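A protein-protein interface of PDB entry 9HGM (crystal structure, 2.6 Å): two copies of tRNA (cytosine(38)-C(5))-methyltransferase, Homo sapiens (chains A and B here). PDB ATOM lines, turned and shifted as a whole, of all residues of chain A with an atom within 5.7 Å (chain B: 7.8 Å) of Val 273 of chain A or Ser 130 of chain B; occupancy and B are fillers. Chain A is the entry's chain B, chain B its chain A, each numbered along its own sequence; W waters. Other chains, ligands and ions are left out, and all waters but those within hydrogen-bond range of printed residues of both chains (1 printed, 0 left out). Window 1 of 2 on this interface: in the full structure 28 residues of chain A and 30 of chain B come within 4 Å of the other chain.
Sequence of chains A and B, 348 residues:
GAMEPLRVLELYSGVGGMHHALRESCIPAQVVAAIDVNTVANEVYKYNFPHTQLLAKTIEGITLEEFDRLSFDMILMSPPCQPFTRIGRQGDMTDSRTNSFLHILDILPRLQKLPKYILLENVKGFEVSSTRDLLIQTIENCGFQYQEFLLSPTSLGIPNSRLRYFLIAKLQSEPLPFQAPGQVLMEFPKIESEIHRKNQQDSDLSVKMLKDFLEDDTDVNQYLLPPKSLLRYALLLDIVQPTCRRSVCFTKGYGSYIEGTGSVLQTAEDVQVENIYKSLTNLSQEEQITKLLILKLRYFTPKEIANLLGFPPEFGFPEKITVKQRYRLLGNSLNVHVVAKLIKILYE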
ATOM      1  N   LEU A 237     -26.467  -3.079   1.738  1.00  0.00           N
ATOM      2  CA  LEU A 237     -25.572  -3.444   2.829  1.00  0.00           C
ATOM      3  C   LEU A 237     -25.358  -2.288   3.793  1.00  0.00           C
ATOM      4  O   LEU A 237     -25.457  -1.107   3.425  1.00  0.00           O
ATOM      5  CB  LEU A 237     -24.216  -3.893   2.270  1.00  0.00           C
ATOM      6  CG  LEU A 237     -24.100  -5.319   1.741  1.00  0.00           C
ATOM      7  CD1 LEU A 237     -22.802  -5.476   0.998  1.00  0.00           C
ATOM      8  CD2 LEU A 237     -24.204  -6.306   2.897  1.00  0.00           C
ATOM      9  N   ILE A 239     -22.386  -0.943   5.428  1.00  0.00           N
ATOM     10  CA  ILE A 239     -20.937  -0.998   5.370  1.00  0.00           C
ATOM     11  C   ILE A 239     -20.371  -0.055   6.420  1.00  0.00           C
ATOM     12  O   ILE A 239     -20.641   1.149   6.391  1.00  0.00           O
ATOM     13  CB  ILE A 239     -20.428  -0.637   3.975  1.00  0.00           C
ATOM     14  CG1 ILE A 239     -21.034  -1.595   2.946  1.00  0.00           C
ATOM     15  CG2 ILE A 239     -18.913  -0.669   3.927  1.00  0.00           C
ATOM     16  CD1 ILE A 239     -20.840  -1.146   1.529  1.00  0.00           C
ATOM     17  N   GLN A 241     -16.729   1.195   8.446  1.00  0.00           N
ATOM     18  CA  GLN A 241     -15.283   1.205   8.332  1.00  0.00           C
ATOM     19  C   GLN A 241     -14.650   1.037   9.704  1.00  0.00           C
ATOM     20  O   GLN A 241     -15.306   1.231  10.732  1.00  0.00           O
ATOM     21  CB  GLN A 241     -14.802   2.511   7.688  1.00  0.00           C
ATOM     22  CG  GLN A 241     -15.475   2.817   6.358  1.00  0.00           C
ATOM     23  CD  GLN A 241     -16.683   3.714   6.511  1.00  0.00           C
ATOM     24  OE1 GLN A 241     -16.659   4.680   7.286  1.00  0.00           O
ATOM     25  NE2 GLN A 241     -17.743   3.408   5.778  1.00  0.00           N
ATOM     26  N   GLN A 266     -15.474  -2.620   5.604  1.00  0.00           N
ATOM     27  CA  GLN A 266     -14.697  -2.183   4.453  1.00  0.00           C
ATOM     28  C   GLN A 266     -13.234  -2.126   4.870  1.00  0.00           C
ATOM     29  O   GLN A 266     -12.832  -1.237   5.630  1.00  0.00           O
ATOM     30  CB  GLN A 266     -15.181  -0.823   3.956  1.00  0.00           C
ATOM     31  CG  GLN A 266     -14.300  -0.192   2.884  1.00  0.00           C
ATOM     32  CD  GLN A 266     -14.597   1.286   2.678  1.00  0.00           C
ATOM     33  OE1 GLN A 266     -15.523   1.838   3.279  1.00  0.00           O
ATOM     34  NE2 GLN A 266     -13.804   1.940   1.831  1.00  0.00           N
ATOM     35  N   VAL A 271     -10.753   4.633  -0.056  1.00  0.00           N
ATOM     36  CA  VAL A 271     -11.795   4.412  -1.045  1.00  0.00           C
ATOM     37  C   VAL A 271     -13.117   4.782  -0.391  1.00  0.00           C
ATOM     38  O   VAL A 271     -13.426   4.304   0.711  1.00  0.00           O
ATOM     39  CB  VAL A 271     -11.812   2.959  -1.544  1.00  0.00           C
ATOM     40  CG1 VAL A 271     -12.901   2.769  -2.595  1.00  0.00           C
ATOM     41  CG2 VAL A 271     -10.473   2.578  -2.105  1.00  0.00           C
ATOM     42  N   GLN A 272     -13.885   5.644  -1.051  1.00  0.00           N
ATOM     43  CA  GLN A 272     -15.129   6.152  -0.497  1.00  0.00           C
ATOM     44  C   GLN A 272     -16.296   5.318  -1.037  1.00  0.00           C
ATOM     45  O   GLN A 272     -16.468   5.197  -2.254  1.00  0.00           O
ATOM     46  CB  GLN A 272     -15.290   7.637  -0.830  1.00  0.00           C
ATOM     47  CG  GLN A 272     -16.480   8.300  -0.149  1.00  0.00           C
ATOM     48  CD  GLN A 272     -16.471   9.809  -0.296  1.00  0.00           C
ATOM     49  OE1 GLN A 272     -15.476  10.406  -0.718  1.00  0.00           O
ATOM     50  NE2 GLN A 272     -17.588  10.435   0.056  1.00  0.00           N
ATOM     51  N   VAL A 273     -17.079   4.746  -0.130  1.00  0.00           N
ATOM     52  CA  VAL A 273     -18.189   3.885  -0.526  1.00  0.00           C
ATOM     53  C   VAL A 273     -19.089   4.605  -1.522  1.00  0.00           C
ATOM     54  O   VAL A 273     -19.446   4.061  -2.575  1.00  0.00           O
ATOM     55  CB  VAL A 273     -18.988   3.426   0.710  1.00  0.00           C
ATOM     56  CG1 VAL A 273     -20.045   2.406   0.316  1.00  0.00           C
ATOM     57  CG2 VAL A 273     -18.047   2.847   1.751  1.00  0.00           C
ATOM     58  N   GLU A 274     -19.466   5.845  -1.203  1.00  0.00           N
ATOM     59  CA  GLU A 274     -20.378   6.580  -2.077  1.00  0.00           C
ATOM     60  C   GLU A 274     -19.803   6.774  -3.472  1.00  0.00           C
ATOM     61  O   GLU A 274     -20.556   6.929  -4.427  1.00  0.00           O
ATOM     62  CB  GLU A 274     -20.727   7.928  -1.452  1.00  0.00           C
ATOM     63  CG  GLU A 274     -21.178   7.816  -0.003  1.00  0.00           C
ATOM     64  CD  GLU A 274     -21.533   9.161   0.612  1.00  0.00           C
ATOM     65  OE1 GLU A 274     -22.035  10.041  -0.123  1.00  0.00           O
ATOM     66  OE2 GLU A 274     -21.307   9.336   1.835  1.00  0.00           O
ATOM     67  N   ASN A 275     -18.469   6.757  -3.613  1.00  0.00           N
ATOM     68  CA  ASN A 275     -17.876   6.879  -4.939  1.00  0.00           C
ATOM     69  C   ASN A 275     -18.030   5.586  -5.729  1.00  0.00           C
ATOM     70  O   ASN A 275     -18.412   5.604  -6.910  1.00  0.00           O
ATOM     71  CB  ASN A 275     -16.407   7.275  -4.823  1.00  0.00           C
ATOM     72  CG  ASN A 275     -16.224   8.736  -4.471  1.00  0.00           C
ATOM     73  OD1 ASN A 275     -17.139   9.382  -3.959  1.00  0.00           O
ATOM     74  ND2 ASN A 275     -15.036   9.266  -4.736  1.00  0.00           N
ATOM     75  N   ILE A 276     -17.738   4.450  -5.102  1.00  0.00           N
ATOM     76  CA  ILE A 276     -18.017   3.159  -5.732  1.00  0.00           C
ATOM     77  C   ILE A 276     -19.486   3.087  -6.147  1.00  0.00           C
ATOM     78  O   ILE A 276     -19.815   2.678  -7.265  1.00  0.00           O
ATOM     79  CB  ILE A 276     -17.641   2.006  -4.786  1.00  0.00           C
ATOM     80  CG1 ILE A 276     -16.126   2.002  -4.541  1.00  0.00           C
ATOM     81  CG2 ILE A 276     -18.091   0.685  -5.359  1.00  0.00           C
ATOM     82  CD1 ILE A 276     -15.322   1.714  -5.789  1.00  0.00           C
ATOM     83  N   TYR A 277     -20.385   3.495  -5.243  1.00  0.00           N
ATOM     84  CA  TYR A 277     -21.814   3.476  -5.537  1.00  0.00           C
ATOM     85  C   TYR A 277     -22.127   4.247  -6.813  1.00  0.00           C
ATOM     86  O   TYR A 277     -22.659   3.690  -7.776  1.00  0.00           O
ATOM     87  CB  TYR A 277     -22.597   4.057  -4.355  1.00  0.00           C
ATOM     88  CG  TYR A 277     -22.854   3.082  -3.223  1.00  0.00           C
ATOM     89  CD1 TYR A 277     -22.441   1.756  -3.307  1.00  0.00           C
ATOM     90  CD2 TYR A 277     -23.534   3.485  -2.079  1.00  0.00           C
ATOM     91  CE1 TYR A 277     -22.688   0.864  -2.278  1.00  0.00           C
ATOM     92  CE2 TYR A 277     -23.782   2.601  -1.042  1.00  0.00           C
ATOM     93  CZ  TYR A 277     -23.362   1.292  -1.152  1.00  0.00           C
ATOM     94  OH  TYR A 277     -23.622   0.407  -0.132  1.00  0.00           O
ATOM     95  N   LYS A 278     -21.788   5.543  -6.838  1.00  0.00           N
ATOM     96  CA  LYS A 278     -22.163   6.375  -7.973  1.00  0.00           C
ATOM     97  C   LYS A 278     -21.528   5.889  -9.267  1.00  0.00           C
ATOM     98  O   LYS A 278     -22.103   6.049 -10.337  1.00  0.00           O
ATOM     99  CB  LYS A 278     -21.785   7.832  -7.703  1.00  0.00           C
ATOM    100  CG  LYS A 278     -22.665   8.850  -8.429  1.00  0.00           C
ATOM    101  CD  LYS A 278     -22.185  10.270  -8.165  1.00  0.00           C
ATOM    102  CE  LYS A 278     -21.903  10.488  -6.680  1.00  0.00           C
ATOM    103  NZ  LYS A 278     -21.510  11.897  -6.405  1.00  0.00           N
ATOM    104  N   LEU A 295     -13.702  -2.091  -2.806  1.00  0.00           N
ATOM    105  CA  LEU A 295     -13.997  -1.746  -1.424  1.00  0.00           C
ATOM    106  C   LEU A 295     -13.421  -2.759  -0.443  1.00  0.00           C
ATOM    107  O   LEU A 295     -13.238  -2.431   0.740  1.00  0.00           O
ATOM    108  CB  LEU A 295     -15.503  -1.623  -1.220  1.00  0.00           C
ATOM    109  CG  LEU A 295     -16.119  -0.334  -1.739  1.00  0.00           C
ATOM    110  CD1 LEU A 295     -17.628  -0.457  -1.716  1.00  0.00           C
ATOM    111  CD2 LEU A 295     -15.657   0.839  -0.887  1.00  0.00           C
ATOM    112  N   PHE B 101     -32.278   2.091  -8.639  1.00  0.00           N
ATOM    113  CA  PHE B 101     -32.022   3.212  -7.733  1.00  0.00           C
ATOM    114  C   PHE B 101     -31.060   4.208  -8.360  1.00  0.00           C
ATOM    115  O   PHE B 101     -31.307   5.418  -8.347  1.00  0.00           O
ATOM    116  CB  PHE B 101     -31.479   2.680  -6.407  1.00  0.00           C
ATOM    117  CG  PHE B 101     -31.055   3.749  -5.441  1.00  0.00           C
ATOM    118  CD1 PHE B 101     -31.991   4.417  -4.673  1.00  0.00           C
ATOM    119  CD2 PHE B 101     -29.709   4.063  -5.282  1.00  0.00           C
ATOM    120  CE1 PHE B 101     -31.607   5.394  -3.780  1.00  0.00           C
ATOM    121  CE2 PHE B 101     -29.313   5.042  -4.384  1.00  0.00           C
ATOM    122  CZ  PHE B 101     -30.264   5.709  -3.633  1.00  0.00           C
ATOM    123  N   GLY B 125     -33.137   1.843  10.066  1.00  0.00           N
ATOM    124  CA  GLY B 125     -31.759   1.532   9.831  1.00  0.00           C
ATOM    125  C   GLY B 125     -31.202   2.181   8.585  1.00  0.00           C
ATOM    126  O   GLY B 125     -30.004   2.485   8.535  1.00  0.00           O
ATOM    127  N   PHE B 126     -32.041   2.419   7.588  1.00  0.00           N
ATOM    128  CA  PHE B 126     -31.592   3.076   6.366  1.00  0.00           C
ATOM    129  C   PHE B 126     -30.934   4.418   6.646  1.00  0.00           C
ATOM    130  O   PHE B 126     -30.007   4.825   5.925  1.00  0.00           O
ATOM    131  CB  PHE B 126     -32.773   3.259   5.410  1.00  0.00           C
ATOM    132  CG  PHE B 126     -32.439   4.029   4.164  1.00  0.00           C
ATOM    133  CD1 PHE B 126     -31.668   3.460   3.155  1.00  0.00           C
ATOM    134  CD2 PHE B 126     -32.910   5.319   3.986  1.00  0.00           C
ATOM    135  CE1 PHE B 126     -31.365   4.169   2.006  1.00  0.00           C
ATOM    136  CE2 PHE B 126     -32.612   6.032   2.843  1.00  0.00           C
ATOM    137  CZ  PHE B 126     -31.840   5.455   1.851  1.00  0.00           C
ATOM    138  N   GLU B 127     -31.375   5.117   7.691  1.00  0.00           N
ATOM    139  CA  GLU B 127     -30.939   6.489   7.926  1.00  0.00           C
ATOM    140  C   GLU B 127     -29.441   6.606   8.256  1.00  0.00           C
ATOM    141  O   GLU B 127     -28.942   7.733   8.354  1.00  0.00           O
ATOM    142  CB  GLU B 127     -31.773   7.111   9.051  1.00  0.00           C
ATOM    143  CG  GLU B 127     -31.564   6.495  10.434  1.00  0.00           C
ATOM    144  CD  GLU B 127     -32.233   5.138  10.599  1.00  0.00           C
ATOM    145  OE1 GLU B 127     -32.661   4.545   9.596  1.00  0.00           O
ATOM    146  OE2 GLU B 127     -32.325   4.658  11.749  1.00  0.00           O
ATOM    147  N   VAL B 128     -28.728   5.499   8.423  1.00  0.00           N
ATOM    148  CA  VAL B 128     -27.293   5.545   8.686  1.00  0.00           C
ATOM    149  C   VAL B 128     -26.495   4.828   7.598  1.00  0.00           C
ATOM    150  O   VAL B 128     -25.354   4.491   7.806  1.00  0.00           O
ATOM    151  CB  VAL B 128     -26.956   4.940  10.056  1.00  0.00           C
ATOM    152  CG1 VAL B 128     -27.871   5.498  11.132  1.00  0.00           C
ATOM    153  CG2 VAL B 128     -27.040   3.420   9.982  1.00  0.00           C
ATOM    154  N   SER B 129     -27.114   4.571   6.447  1.00  0.00           N
ATOM    155  CA  SER B 129     -26.454   3.797   5.404  1.00  0.00           C
ATOM    156  C   SER B 129     -25.682   4.703   4.459  1.00  0.00           C
ATOM    157  O   SER B 129     -26.027   5.870   4.262  1.00  0.00           O
ATOM    158  CB  SER B 129     -27.485   2.980   4.619  1.00  0.00           C
ATOM    159  OG  SER B 129     -28.380   3.824   3.912  1.00  0.00           O
ATOM    160  N   SER B 130     -24.629   4.152   3.862  1.00  0.00           N
ATOM    161  CA  SER B 130     -23.960   4.882   2.787  1.00  0.00           C
ATOM    162  C   SER B 130     -24.932   5.213   1.665  1.00  0.00           C
ATOM    163  O   SER B 130     -24.793   6.242   0.998  1.00  0.00           O
ATOM    164  CB  SER B 130     -22.784   4.069   2.252  1.00  0.00           C
ATOM    165  OG  SER B 130     -21.828   3.852   3.271  1.00  0.00           O
ATOM    166  N   THR B 131     -25.936   4.359   1.453  1.00  0.00           N
ATOM    167  CA  THR B 131     -26.903   4.615   0.387  1.00  0.00           C
ATOM    168  C   THR B 131     -27.687   5.898   0.660  1.00  0.00           C
ATOM    169  O   THR B 131     -27.824   6.754  -0.223  1.00  0.00           O
ATOM    170  CB  THR B 131     -27.841   3.422   0.230  1.00  0.00           C
ATOM    171  OG1 THR B 131     -27.070   2.245  -0.005  1.00  0.00           O
ATOM    172  CG2 THR B 131     -28.768   3.639  -0.941  1.00  0.00           C
ATOM    173  N   ARG B 132     -28.208   6.053   1.883  1.00  0.00           N
ATOM    174  CA  ARG B 132     -28.905   7.281   2.233  1.00  0.00           C
ATOM    175  C   ARG B 132     -28.053   8.503   1.925  1.00  0.00           C
ATOM    176  O   ARG B 132     -28.556   9.504   1.390  1.00  0.00           O
ATOM    177  CB  ARG B 132     -29.284   7.270   3.714  1.00  0.00           C
ATOM    178  CG  ARG B 132     -29.766   8.633   4.207  1.00  0.00           C
ATOM    179  CD  ARG B 132     -29.141   9.008   5.531  1.00  0.00           C
ATOM    180  NE  ARG B 132     -29.494  10.367   5.932  1.00  0.00           N
ATOM    181  CZ  ARG B 132     -28.741  11.433   5.714  1.00  0.00           C
ATOM    182  NH1 ARG B 132     -27.568  11.339   5.104  1.00  0.00           N
ATOM    183  NH2 ARG B 132     -29.174  12.625   6.114  1.00  0.00           N
ATOM    184  N   ASP B 133     -26.756   8.435   2.258  1.00  0.00           N
ATOM    185  CA  ASP B 133     -25.864   9.566   2.028  1.00  0.00           C
ATOM    186  C   ASP B 133     -25.832   9.950   0.556  1.00  0.00           C
ATOM    187  O   ASP B 133     -25.920  11.134   0.211  1.00  0.00           O
ATOM    188  CB  ASP B 133     -24.455   9.235   2.530  1.00  0.00           C
ATOM    189  CG  ASP B 133     -24.373   9.115   4.053  1.00  0.00           C
ATOM    190  OD1 ASP B 133     -25.254   9.647   4.755  1.00  0.00           O
ATOM    191  OD2 ASP B 133     -23.402   8.502   4.554  1.00  0.00           O
ATOM    192  N   LEU B 134     -25.696   8.957  -0.332  1.00  0.00           N
ATOM    193  CA  LEU B 134     -25.710   9.246  -1.764  1.00  0.00           C
ATOM    194  C   LEU B 134     -27.070   9.778  -2.197  1.00  0.00           C
ATOM    195  O   LEU B 134     -27.162  10.654  -3.064  1.00  0.00           O
ATOM    196  CB  LEU B 134     -25.342   7.992  -2.547  1.00  0.00           C
ATOM    197  CG  LEU B 134     -25.332   8.121  -4.068  1.00  0.00           C
ATOM    198  CD1 LEU B 134     -24.167   8.992  -4.543  1.00  0.00           C
ATOM    199  CD2 LEU B 134     -25.300   6.747  -4.726  1.00  0.00           C
ATOM    200  N   LEU B 135     -28.143   9.261  -1.598  1.00  0.00           N
ATOM    201  CA  LEU B 135     -29.483   9.759  -1.900  1.00  0.00           C
ATOM    202  C   LEU B 135     -29.642  11.205  -1.468  1.00  0.00           C
ATOM    203  O   LEU B 135     -30.093  12.052  -2.253  1.00  0.00           O
ATOM    204  CB  LEU B 135     -30.529   8.876  -1.224  1.00  0.00           C
ATOM    205  CG  LEU B 135     -31.952   9.442  -1.177  1.00  0.00           C
ATOM    206  CD1 LEU B 135     -32.549   9.542  -2.571  1.00  0.00           C
ATOM    207  CD2 LEU B 135     -32.821   8.582  -0.279  1.00  0.00           C
ATOM    208  N   ILE B 136     -29.296  11.508  -0.209  1.00  0.00           N
ATOM    209  CA  ILE B 136     -29.413  12.875   0.306  1.00  0.00           C
ATOM    210  C   ILE B 136     -28.584  13.828  -0.540  1.00  0.00           C
ATOM    211  O   ILE B 136     -29.044  14.910  -0.926  1.00  0.00           O
ATOM    212  CB  ILE B 136     -28.989  12.925   1.783  1.00  0.00           C
ATOM    213  CG1 ILE B 136     -30.000  12.174   2.649  1.00  0.00           C
ATOM    214  CG2 ILE B 136     -28.848  14.359   2.247  1.00  0.00           C
ATOM    215  CD1 ILE B 136     -31.312  12.884   2.801  1.00  0.00           C
HETATM  216  O   HOH W   1     -24.272   1.806   5.971  1.00  0.00           O
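Printed residues of chain A that touch a printed residue of chain B: Val 273, Glu 274, Tyr 277 and Lys 278.
Hydrophobic or aromatic side chains of chain A within 4 Å of the printed part of chain B: Val 273 and Tyr 277.
Of the 13 printed residues of chain B, 4 touch a printed residue of chain A.
Printed residues of chain B that touch a printed residue of chain A: Ser 130, Thr 131, Asp 133 and Leu 134.
Hydrophobic or aromatic side chains of chain B that line the printed part of chain A: Leu 134.
Along chain B the printed residues that touch a printed residue of chain A span positions 130 to 134.
Printed residues of chain B within 4 Å of Val 273 of chain A: Ser 130 (3.7 Å).
Of the printed residues of chain B, Tyr 277 of chain A touches Ser 130, Thr 131 and Leu 134.
Phe 101 of chain B touches none of the printed residues of chain A.
Glu 127 of chain B touches none of the printed residues of chain A.
Ser 130 of chain B touches just these residues of chain A: Val 273 and Tyr 277.
Of the printed residues of chain A, Thr 131 of chain B touches Tyr 277.
Printed residues of chain A within 4 Å of Leu 134 of chain B: Glu 274, Tyr 277 and Lys 278.
Ser 130 of chain B touches Val 273 of chain A (OG to CG1, 3.7 Å).
Glu 274 of chain A touches Asp 133 of chain B.
N of Leu 134 of chain B touches OE1 of Glu 274 of chain A, 3.8 Å away.
Ser 130 of chain B touches Tyr 277 of chain A.
OG1 of Thr 131 of chain B touches CE2 of Tyr 277 of chain A, at 3.5 Å.
Tyr 277 of chain A touches Leu 134 of chain B (CB to CD2, 3.8 Å).
CE of Lys 278 of chain A touches CD1 of Leu 134 of chain B (3.5 Å).
No position is printed for both chains.
Of the 7 pairs that touch across the chains among the printed residues, none has its exchanged pair printed and touching as well.
Water W1 lies within hydrogen-bond range of N of Ser 130 of chain B (3.2 Å), N of Ile 239 of chain A (3.4 Å) and O of Val 128 of chain B (3.4 Å).
The guanidinium group (NH1) of Arg 132 of chain B lies within salt-bridge range of the side-chain carboxylate (OD1) of Asp 133 of chain B (2.9 Å).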
